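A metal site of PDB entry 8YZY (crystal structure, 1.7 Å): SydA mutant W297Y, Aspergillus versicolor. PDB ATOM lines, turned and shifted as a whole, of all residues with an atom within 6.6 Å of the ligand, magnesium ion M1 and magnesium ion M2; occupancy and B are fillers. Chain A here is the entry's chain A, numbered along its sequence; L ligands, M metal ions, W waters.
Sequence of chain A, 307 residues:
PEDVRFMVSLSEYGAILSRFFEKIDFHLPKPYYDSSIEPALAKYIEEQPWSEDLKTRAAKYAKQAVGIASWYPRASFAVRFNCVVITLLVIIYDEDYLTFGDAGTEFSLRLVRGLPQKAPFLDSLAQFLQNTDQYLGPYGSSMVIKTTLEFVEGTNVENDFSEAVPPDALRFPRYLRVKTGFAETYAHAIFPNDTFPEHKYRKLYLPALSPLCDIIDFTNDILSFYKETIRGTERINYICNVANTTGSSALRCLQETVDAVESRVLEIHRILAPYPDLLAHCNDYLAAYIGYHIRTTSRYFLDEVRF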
ATOM      1  N   ASP A  94      32.133   8.218  -6.484  1.00  0.00           N
ATOM      2  CA  ASP A  94      30.794   8.421  -5.890  1.00  0.00           C
ATOM      3  C   ASP A  94      29.777   8.762  -6.943  1.00  0.00           C
ATOM      4  O   ASP A  94      28.585   8.477  -6.759  1.00  0.00           O
ATOM      5  CB  ASP A  94      30.806   9.599  -4.865  1.00  0.00           C
ATOM      6  CG  ASP A  94      29.681   9.496  -3.760  1.00  0.00           C
ATOM      7  OD1 ASP A  94      29.689   8.490  -2.986  1.00  0.00           O
ATOM      8  OD2 ASP A  94      28.818  10.426  -3.629  1.00  0.00           O
ATOM      9  N   GLU A  95      30.207   9.386  -8.044  1.00  0.00           N
ATOM     10  CA  GLU A  95      29.302   9.781  -9.120  1.00  0.00           C
ATOM     11  C   GLU A  95      29.308   8.819 -10.293  1.00  0.00           C
ATOM     12  O   GLU A  95      28.250   8.562 -10.871  1.00  0.00           O
ATOM     13  CB  GLU A  95      29.638  11.196  -9.622  1.00  0.00           C
ATOM     14  CG  GLU A  95      29.498  12.245  -8.532  1.00  0.00           C
ATOM     15  CD  GLU A  95      28.065  12.511  -8.114  1.00  0.00           C
ATOM     16  OE1 GLU A  95      27.126  11.920  -8.694  1.00  0.00           O
ATOM     17  OE2 GLU A  95      27.885  13.283  -7.131  1.00  0.00           O
ATOM     18  N   PHE A 151      34.987   2.139   1.663  1.00  0.00           N
ATOM     19  CA  PHE A 151      34.225   3.050   0.811  1.00  0.00           C
ATOM     20  C   PHE A 151      33.946   2.448  -0.559  1.00  0.00           C
ATOM     21  O   PHE A 151      32.837   2.592  -1.102  1.00  0.00           O
ATOM     22  CB  PHE A 151      34.999   4.368   0.667  1.00  0.00           C
ATOM     23  CG  PHE A 151      34.457   5.253  -0.423  1.00  0.00           C
ATOM     24  CD1 PHE A 151      33.300   6.020  -0.227  1.00  0.00           C
ATOM     25  CD2 PHE A 151      35.073   5.294  -1.655  1.00  0.00           C
ATOM     26  CE1 PHE A 151      32.780   6.811  -1.276  1.00  0.00           C
ATOM     27  CE2 PHE A 151      34.576   6.084  -2.706  1.00  0.00           C
ATOM     28  CZ  PHE A 151      33.419   6.851  -2.509  1.00  0.00           C
ATOM     29  N   GLU A 158      25.593  -0.264  -1.638  1.00  0.00           N
ATOM     30  CA  GLU A 158      24.552   0.681  -1.192  1.00  0.00           C
ATOM     31  C   GLU A 158      23.185   0.455  -1.818  1.00  0.00           C
ATOM     32  O   GLU A 158      22.157   0.365  -1.124  1.00  0.00           O
ATOM     33  CB  GLU A 158      25.015   2.089  -1.584  1.00  0.00           C
ATOM     34  CG  GLU A 158      25.305   3.000  -0.488  1.00  0.00           C
ATOM     35  CD  GLU A 158      25.664   4.367  -1.014  1.00  0.00           C
ATOM     36  OE1 GLU A 158      26.390   4.454  -2.052  1.00  0.00           O
ATOM     37  OE2 GLU A 158      25.231   5.343  -0.377  1.00  0.00           O
ATOM     38  N   ARG A 177      26.502   3.388   6.882  1.00  0.00           N
ATOM     39  CA  ARG A 177      27.022   4.740   6.800  1.00  0.00           C
ATOM     40  C   ARG A 177      28.504   4.780   7.151  1.00  0.00           C
ATOM     41  O   ARG A 177      29.257   5.557   6.559  1.00  0.00           O
ATOM     42  CB  ARG A 177      26.204   5.687   7.706  1.00  0.00           C
ATOM     43  CG  ARG A 177      26.692   7.142   7.657  1.00  0.00           C
ATOM     44  CD  ARG A 177      26.812   7.602   6.162  1.00  0.00           C
ATOM     45  NE  ARG A 177      26.777   9.043   6.007  1.00  0.00           N
ATOM     46  CZ  ARG A 177      27.194   9.678   4.910  1.00  0.00           C
ATOM     47  NH1 ARG A 177      27.680   9.008   3.877  1.00  0.00           N
ATOM     48  NH2 ARG A 177      27.128  11.007   4.864  1.00  0.00           N
ATOM     49  N   THR A 180      30.141   3.775   3.849  1.00  0.00           N
ATOM     50  CA  THR A 180      30.066   4.706   2.726  1.00  0.00           C
ATOM     51  C   THR A 180      30.627   6.104   3.019  1.00  0.00           C
ATOM     52  O   THR A 180      30.920   6.853   2.074  1.00  0.00           O
ATOM     53  CB  THR A 180      28.611   4.888   2.270  1.00  0.00           C
ATOM     54  OG1 THR A 180      27.864   5.497   3.324  1.00  0.00           O
ATOM     55  CG2 THR A 180      28.011   3.563   1.916  1.00  0.00           C
ATOM     56  N   GLY A 181      30.788   6.479   4.292  1.00  0.00           N
ATOM     57  CA  GLY A 181      31.072   7.863   4.596  1.00  0.00           C
ATOM     58  C   GLY A 181      32.501   8.315   4.419  1.00  0.00           C
ATOM     59  O   GLY A 181      32.738   9.518   4.363  1.00  0.00           O
ATOM     60  N   PHE A 182      33.459   7.390   4.386  1.00  0.00           N
ATOM     61  CA  PHE A 182      34.870   7.759   4.155  1.00  0.00           C
ATOM     62  C   PHE A 182      35.413   8.664   5.270  1.00  0.00           C
ATOM     63  O   PHE A 182      36.400   9.392   5.088  1.00  0.00           O
ATOM     64  CB  PHE A 182      35.019   8.419   2.772  1.00  0.00           C
ATOM     65  CG  PHE A 182      36.385   8.306   2.186  1.00  0.00           C
ATOM     66  CD1 PHE A 182      36.966   7.058   1.973  1.00  0.00           C
ATOM     67  CD2 PHE A 182      37.085   9.453   1.811  1.00  0.00           C
ATOM     68  CE1 PHE A 182      38.239   6.962   1.395  1.00  0.00           C
ATOM     69  CE2 PHE A 182      38.368   9.367   1.235  1.00  0.00           C
ATOM     70  CZ  PHE A 182      38.940   8.117   1.026  1.00  0.00           C
ATOM     71  N   ASP A 217      30.202  12.045   9.177  1.00  0.00           N
ATOM     72  CA  ASP A 217      29.147  11.307   8.475  1.00  0.00           C
ATOM     73  C   ASP A 217      27.802  12.015   8.611  1.00  0.00           C
ATOM     74  O   ASP A 217      27.141  12.369   7.606  1.00  0.00           O
ATOM     75  CB  ASP A 217      29.022   9.888   9.071  1.00  0.00           C
ATOM     76  CG  ASP A 217      30.122   8.932   8.646  1.00  0.00           C
ATOM     77  OD1 ASP A 217      30.854   9.218   7.675  1.00  0.00           O
ATOM     78  OD2 ASP A 217      30.233   7.859   9.292  1.00  0.00           O
ATOM     79  N   ASN A 220      27.230  15.599   7.064  1.00  0.00           N
ATOM     80  CA  ASN A 220      26.884  15.492   5.654  1.00  0.00           C
ATOM     81  C   ASN A 220      25.464  14.973   5.477  1.00  0.00           C
ATOM     82  O   ASN A 220      24.705  15.456   4.617  1.00  0.00           O
ATOM     83  CB  ASN A 220      27.859  14.609   4.908  1.00  0.00           C
ATOM     84  CG  ASN A 220      27.372  14.350   3.507  1.00  0.00           C
ATOM     85  OD1 ASN A 220      26.648  13.383   3.294  1.00  0.00           O
ATOM     86  ND2 ASN A 220      27.680  15.251   2.556  1.00  0.00           N
ATOM     87  N   ASP A 221      25.044  13.975   6.271  1.00  0.00           N
ATOM     88  CA  ASP A 221      23.660  13.506   6.123  1.00  0.00           C
ATOM     89  C   ASP A 221      22.658  14.657   6.296  1.00  0.00           C
ATOM     90  O   ASP A 221      21.740  14.816   5.480  1.00  0.00           O
ATOM     91  CB  ASP A 221      23.374  12.361   7.083  1.00  0.00           C
ATOM     92  CG  ASP A 221      24.087  11.056   6.671  1.00  0.00           C
ATOM     93  OD1 ASP A 221      23.958  10.629   5.481  1.00  0.00           O
ATOM     94  OD2 ASP A 221      24.797  10.438   7.503  1.00  0.00           O
ATOM     95  N   LEU A 223      23.165  17.987   5.945  1.00  0.00           N
ATOM     96  CA  LEU A 223      23.298  19.089   5.000  1.00  0.00           C
ATOM     97  C   LEU A 223      23.122  18.644   3.551  1.00  0.00           C
ATOM     98  O   LEU A 223      22.906  19.470   2.664  1.00  0.00           O
ATOM     99  CB  LEU A 223      24.685  19.737   5.157  1.00  0.00           C
ATOM    100  CG  LEU A 223      24.869  20.379   6.539  1.00  0.00           C
ATOM    101  CD1 LEU A 223      26.266  20.920   6.706  1.00  0.00           C
ATOM    102  CD2 LEU A 223      23.785  21.467   6.794  1.00  0.00           C
ATOM    103  N   SER A 224      23.254  17.356   3.274  1.00  0.00           N
ATOM    104  CA  SER A 224      23.009  16.854   1.931  1.00  0.00           C
ATOM    105  C   SER A 224      21.636  16.214   1.829  1.00  0.00           C
ATOM    106  O   SER A 224      21.298  15.725   0.739  1.00  0.00           O
ATOM    107  CB  SER A 224      24.107  15.853   1.501  1.00  0.00           C
ATOM    108  OG  SER A 224      24.091  14.664   2.292  1.00  0.00           O
ATOM    109  N   PHE A 225      20.840  16.205   2.906  1.00  0.00           N
ATOM    110  CA  PHE A 225      19.498  15.659   2.755  1.00  0.00           C
ATOM    111  C   PHE A 225      18.702  16.381   1.672  1.00  0.00           C
ATOM    112  O   PHE A 225      17.896  15.740   0.987  1.00  0.00           O
ATOM    113  CB  PHE A 225      18.737  15.722   4.071  1.00  0.00           C
ATOM    114  CG  PHE A 225      17.424  15.008   4.027  1.00  0.00           C
ATOM    115  CD1 PHE A 225      17.380  13.617   4.074  1.00  0.00           C
ATOM    116  CD2 PHE A 225      16.245  15.705   3.963  1.00  0.00           C
ATOM    117  CE1 PHE A 225      16.162  12.947   4.057  1.00  0.00           C
ATOM    118  CE2 PHE A 225      15.022  15.041   3.940  1.00  0.00           C
ATOM    119  CZ  PHE A 225      14.973  13.663   3.986  1.00  0.00           C
ATOM    120  N   LYS A 227      19.769  17.768  -1.270  1.00  0.00           N
ATOM    121  CA  LYS A 227      20.103  17.362  -2.628  1.00  0.00           C
ATOM    122  C   LYS A 227      19.827  15.883  -2.853  1.00  0.00           C
ATOM    123  O   LYS A 227      19.520  15.468  -3.980  1.00  0.00           O
ATOM    124  CB  LYS A 227      21.556  17.727  -2.981  1.00  0.00           C
ATOM    125  CG  LYS A 227      22.676  16.881  -2.273  1.00  0.00           C
ATOM    126  CD  LYS A 227      23.166  15.726  -3.184  1.00  0.00           C
ATOM    127  CE  LYS A 227      24.408  15.087  -2.560  1.00  0.00           C
ATOM    128  NZ  LYS A 227      24.840  13.898  -3.398  1.00  0.00           N
ATOM    129  N   GLU A 228      19.898  15.072  -1.792  1.00  0.00           N
ATOM    130  CA  GLU A 228      19.685  13.636  -1.984  1.00  0.00           C
ATOM    131  C   GLU A 228      18.198  13.311  -2.060  1.00  0.00           C
ATOM    132  O   GLU A 228      17.754  12.619  -2.987  1.00  0.00           O
ATOM    133  CB  GLU A 228      20.338  12.862  -0.825  1.00  0.00           C
ATOM    134  CG  GLU A 228      21.826  12.947  -0.913  1.00  0.00           C
ATOM    135  CD  GLU A 228      22.558  12.451   0.294  1.00  0.00           C
ATOM    136  OE1 GLU A 228      21.923  12.049   1.308  1.00  0.00           O
ATOM    137  OE2 GLU A 228      23.807  12.474   0.225  1.00  0.00           O
ATOM    138  N   GLU A 234      17.376   9.971  -4.047  1.00  0.00           N
ATOM    139  CA  GLU A 234      18.091   9.016  -3.196  1.00  0.00           C
ATOM    140  C   GLU A 234      17.237   8.645  -1.985  1.00  0.00           C
ATOM    141  O   GLU A 234      16.806   9.526  -1.234  1.00  0.00           O
ATOM    142  CB  GLU A 234      19.450   9.587  -2.772  1.00  0.00           C
ATOM    143  CG  GLU A 234      20.409   8.582  -2.077  1.00  0.00           C
ATOM    144  CD  GLU A 234      21.852   9.108  -1.896  1.00  0.00           C
ATOM    145  OE1 GLU A 234      22.280   9.982  -2.692  1.00  0.00           O
ATOM    146  OE2 GLU A 234      22.563   8.655  -0.933  1.00  0.00           O
ATOM    147  N   ASN A 237      19.980   6.528   1.621  1.00  0.00           N
ATOM    148  CA  ASN A 237      20.939   7.176   2.496  1.00  0.00           C
ATOM    149  C   ASN A 237      20.627   6.850   3.956  1.00  0.00           C
ATOM    150  O   ASN A 237      19.635   6.184   4.294  1.00  0.00           O
ATOM    151  CB  ASN A 237      20.989   8.671   2.220  1.00  0.00           C
ATOM    152  CG  ASN A 237      19.612   9.336   2.316  1.00  0.00           C
ATOM    153  OD1 ASN A 237      18.683   8.781   2.903  1.00  0.00           O
ATOM    154  ND2 ASN A 237      19.486  10.497   1.707  1.00  0.00           N
ATOM    155  N   HIS A 293      29.759  22.741   2.755  1.00  0.00           N
ATOM    156  CA  HIS A 293      28.446  22.299   2.284  1.00  0.00           C
ATOM    157  C   HIS A 293      27.580  23.474   1.836  1.00  0.00           C
ATOM    158  O   HIS A 293      26.816  23.365   0.870  1.00  0.00           O
ATOM    159  CB  HIS A 293      27.716  21.520   3.372  1.00  0.00           C
ATOM    160  CG  HIS A 293      28.221  20.127   3.524  1.00  0.00           C
ATOM    161  ND1 HIS A 293      29.370  19.837   4.230  1.00  0.00           N
ATOM    162  CD2 HIS A 293      27.740  18.935   3.088  1.00  0.00           C
ATOM    163  CE1 HIS A 293      29.594  18.518   4.186  1.00  0.00           C
ATOM    164  NE2 HIS A 293      28.612  17.951   3.510  1.00  0.00           N
ATOM    165  N   ARG A 299      26.962  21.186  -5.652  1.00  0.00           N
ATOM    166  CA  ARG A 299      26.801  19.831  -5.140  1.00  0.00           C
ATOM    167  C   ARG A 299      25.630  19.690  -4.165  1.00  0.00           C
ATOM    168  O   ARG A 299      24.909  18.682  -4.236  1.00  0.00           O
ATOM    169  CB  ARG A 299      28.114  19.364  -4.473  1.00  0.00           C
ATOM    170  CG  ARG A 299      28.134  17.874  -4.214  1.00  0.00           C
ATOM    171  CD  ARG A 299      29.424  17.333  -3.561  1.00  0.00           C
ATOM    172  NE  ARG A 299      29.308  15.885  -3.391  1.00  0.00           N
ATOM    173  CZ  ARG A 299      29.308  15.001  -4.379  1.00  0.00           C
ATOM    174  NH1 ARG A 299      29.555  15.368  -5.628  1.00  0.00           N
ATOM    175  NH2 ARG A 299      29.020  13.738  -4.113  1.00  0.00           N
ATOM    176  N   TYR A 300      25.377  20.690  -3.298  1.00  0.00           N
ATOM    177  CA  TYR A 300      24.345  20.587  -2.259  1.00  0.00           C
ATOM    178  C   TYR A 300      23.179  21.539  -2.437  1.00  0.00           C
ATOM    179  O   TYR A 300      22.148  21.350  -1.777  1.00  0.00           O
ATOM    180  CB  TYR A 300      24.947  20.806  -0.855  1.00  0.00           C
ATOM    181  CG  TYR A 300      26.067  19.806  -0.654  1.00  0.00           C
ATOM    182  CD1 TYR A 300      25.792  18.455  -0.542  1.00  0.00           C
ATOM    183  CD2 TYR A 300      27.419  20.210  -0.668  1.00  0.00           C
ATOM    184  CE1 TYR A 300      26.833  17.508  -0.403  1.00  0.00           C
ATOM    185  CE2 TYR A 300      28.474  19.267  -0.520  1.00  0.00           C
ATOM    186  CZ  TYR A 300      28.162  17.929  -0.386  1.00  0.00           C
ATOM    187  OH  TYR A 300      29.152  16.981  -0.255  1.00  0.00           O
HETATM  188  P1  LIG L   1      27.482  13.517  -0.603  1.00  0.00           P
HETATM  189  O1  LIG L   1      26.997  12.797  -1.847  1.00  0.00           O
HETATM  190  O2  LIG L   1      26.391  14.000   0.302  1.00  0.00           O
HETATM  191  O3  LIG L   1      28.463  14.600  -0.864  1.00  0.00           O
HETATM  192  O4  LIG L   1      28.329  12.385   0.217  1.00  0.00           O
HETATM  193  P2  LIG L   1      27.712  10.946   0.606  1.00  0.00           P
HETATM  194  O5  LIG L   1      26.394  11.160   1.268  1.00  0.00           O
HETATM  195  O6  LIG L   1      27.596  10.106  -0.631  1.00  0.00           O
HETATM  196  O7  LIG L   1      28.713  10.341   1.563  1.00  0.00           O
HETATM  197 MG    MG M   1      25.344  12.854   1.690  1.00  0.00          MG
HETATM  198 MG    MG M   2      26.764  10.728  -2.444  1.00  0.00          MG
HETATM  199  O   HOH W   1      24.740   9.034   1.379  1.00  0.00           O
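O7 of the ligand lies within salt-bridge range of NH1 of Arg 177 (2.9 Å). An oxygen (O1) of the ligand lies close to the side-chain amino group of Lys 227 (2.9 Å). The guanidinium group (NE) of Arg 299 is in salt-bridge range of an oxygen (O3) of the ligand, at 3.0 Å. OH of Tyr 300 lies within hydrogen-bond range of O3 of the ligand (2.6 Å).
The side-chain amide nitrogen of Asn 220 lies within hydrogen-bond range of a ring nitrogen (NE2) of His 293 (3.0 Å). The guanidinium group (NE) of Arg 177 lies within salt-bridge range of the side-chain carboxylate (OD2) of Asp 221, 2.8 Å away. NH1 of Arg 299 is in salt-bridge range of OE2 of Glu 95, 3.1 Å away. The guanidinium group (NH2) of Arg 177 sits close to the side-chain amide oxygen (OD1) of Asn 220, at 2.9 Å. The side-chain carboxylate (OE1) of Glu 228 lies within hydrogen-bond range of the side-chain amide nitrogen (ND2) of Asn 237, at 2.9 Å. The side-chain hydroxyl of Tyr 300 sits at hydrogen-bond distance from the guanidinium group of Arg 299. The side-chain carboxylate of Asp 94 lies close to the guanidinium group of Arg 299 (3.4 Å). O of Asp 217 sits at hydrogen-bond distance from NH2 of Arg 177, at 3.1 Å.
Three residues have an atom within 4 Å of magnesium ion M1: Asn 220, Ser 224 and Glu 228.
Lys 227 touches magnesium ion M2. Within 4 Å of magnesium ion M2: Asp 94 and Lys 227. The nearest printed residue that does not touch magnesium ion M2 is Arg 299 (4.1 Å).
Magnesium ion M1 is bound by O5 of the ligand (2.0 Å), O2 of the ligand (2.1 Å), OD1 of Asn 220 (2.1 Å), OE2 of Glu 228 (2.2 Å) and OG of Ser 224 (2.3 Å). Magnesium ion M1 has five donor atoms within binding distance.
Magnesium ion M2 is bound by O6 of the ligand, 2.1 Å away. An oxygen (O1) of the ligand is bound to magnesium ion M2, 2.2 Å away. The side-chain carboxylate (OD2) of Asp 94 binds magnesium ion M2, 2.4 Å away. Magnesium ion M2 has three donor atoms within binding distance.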
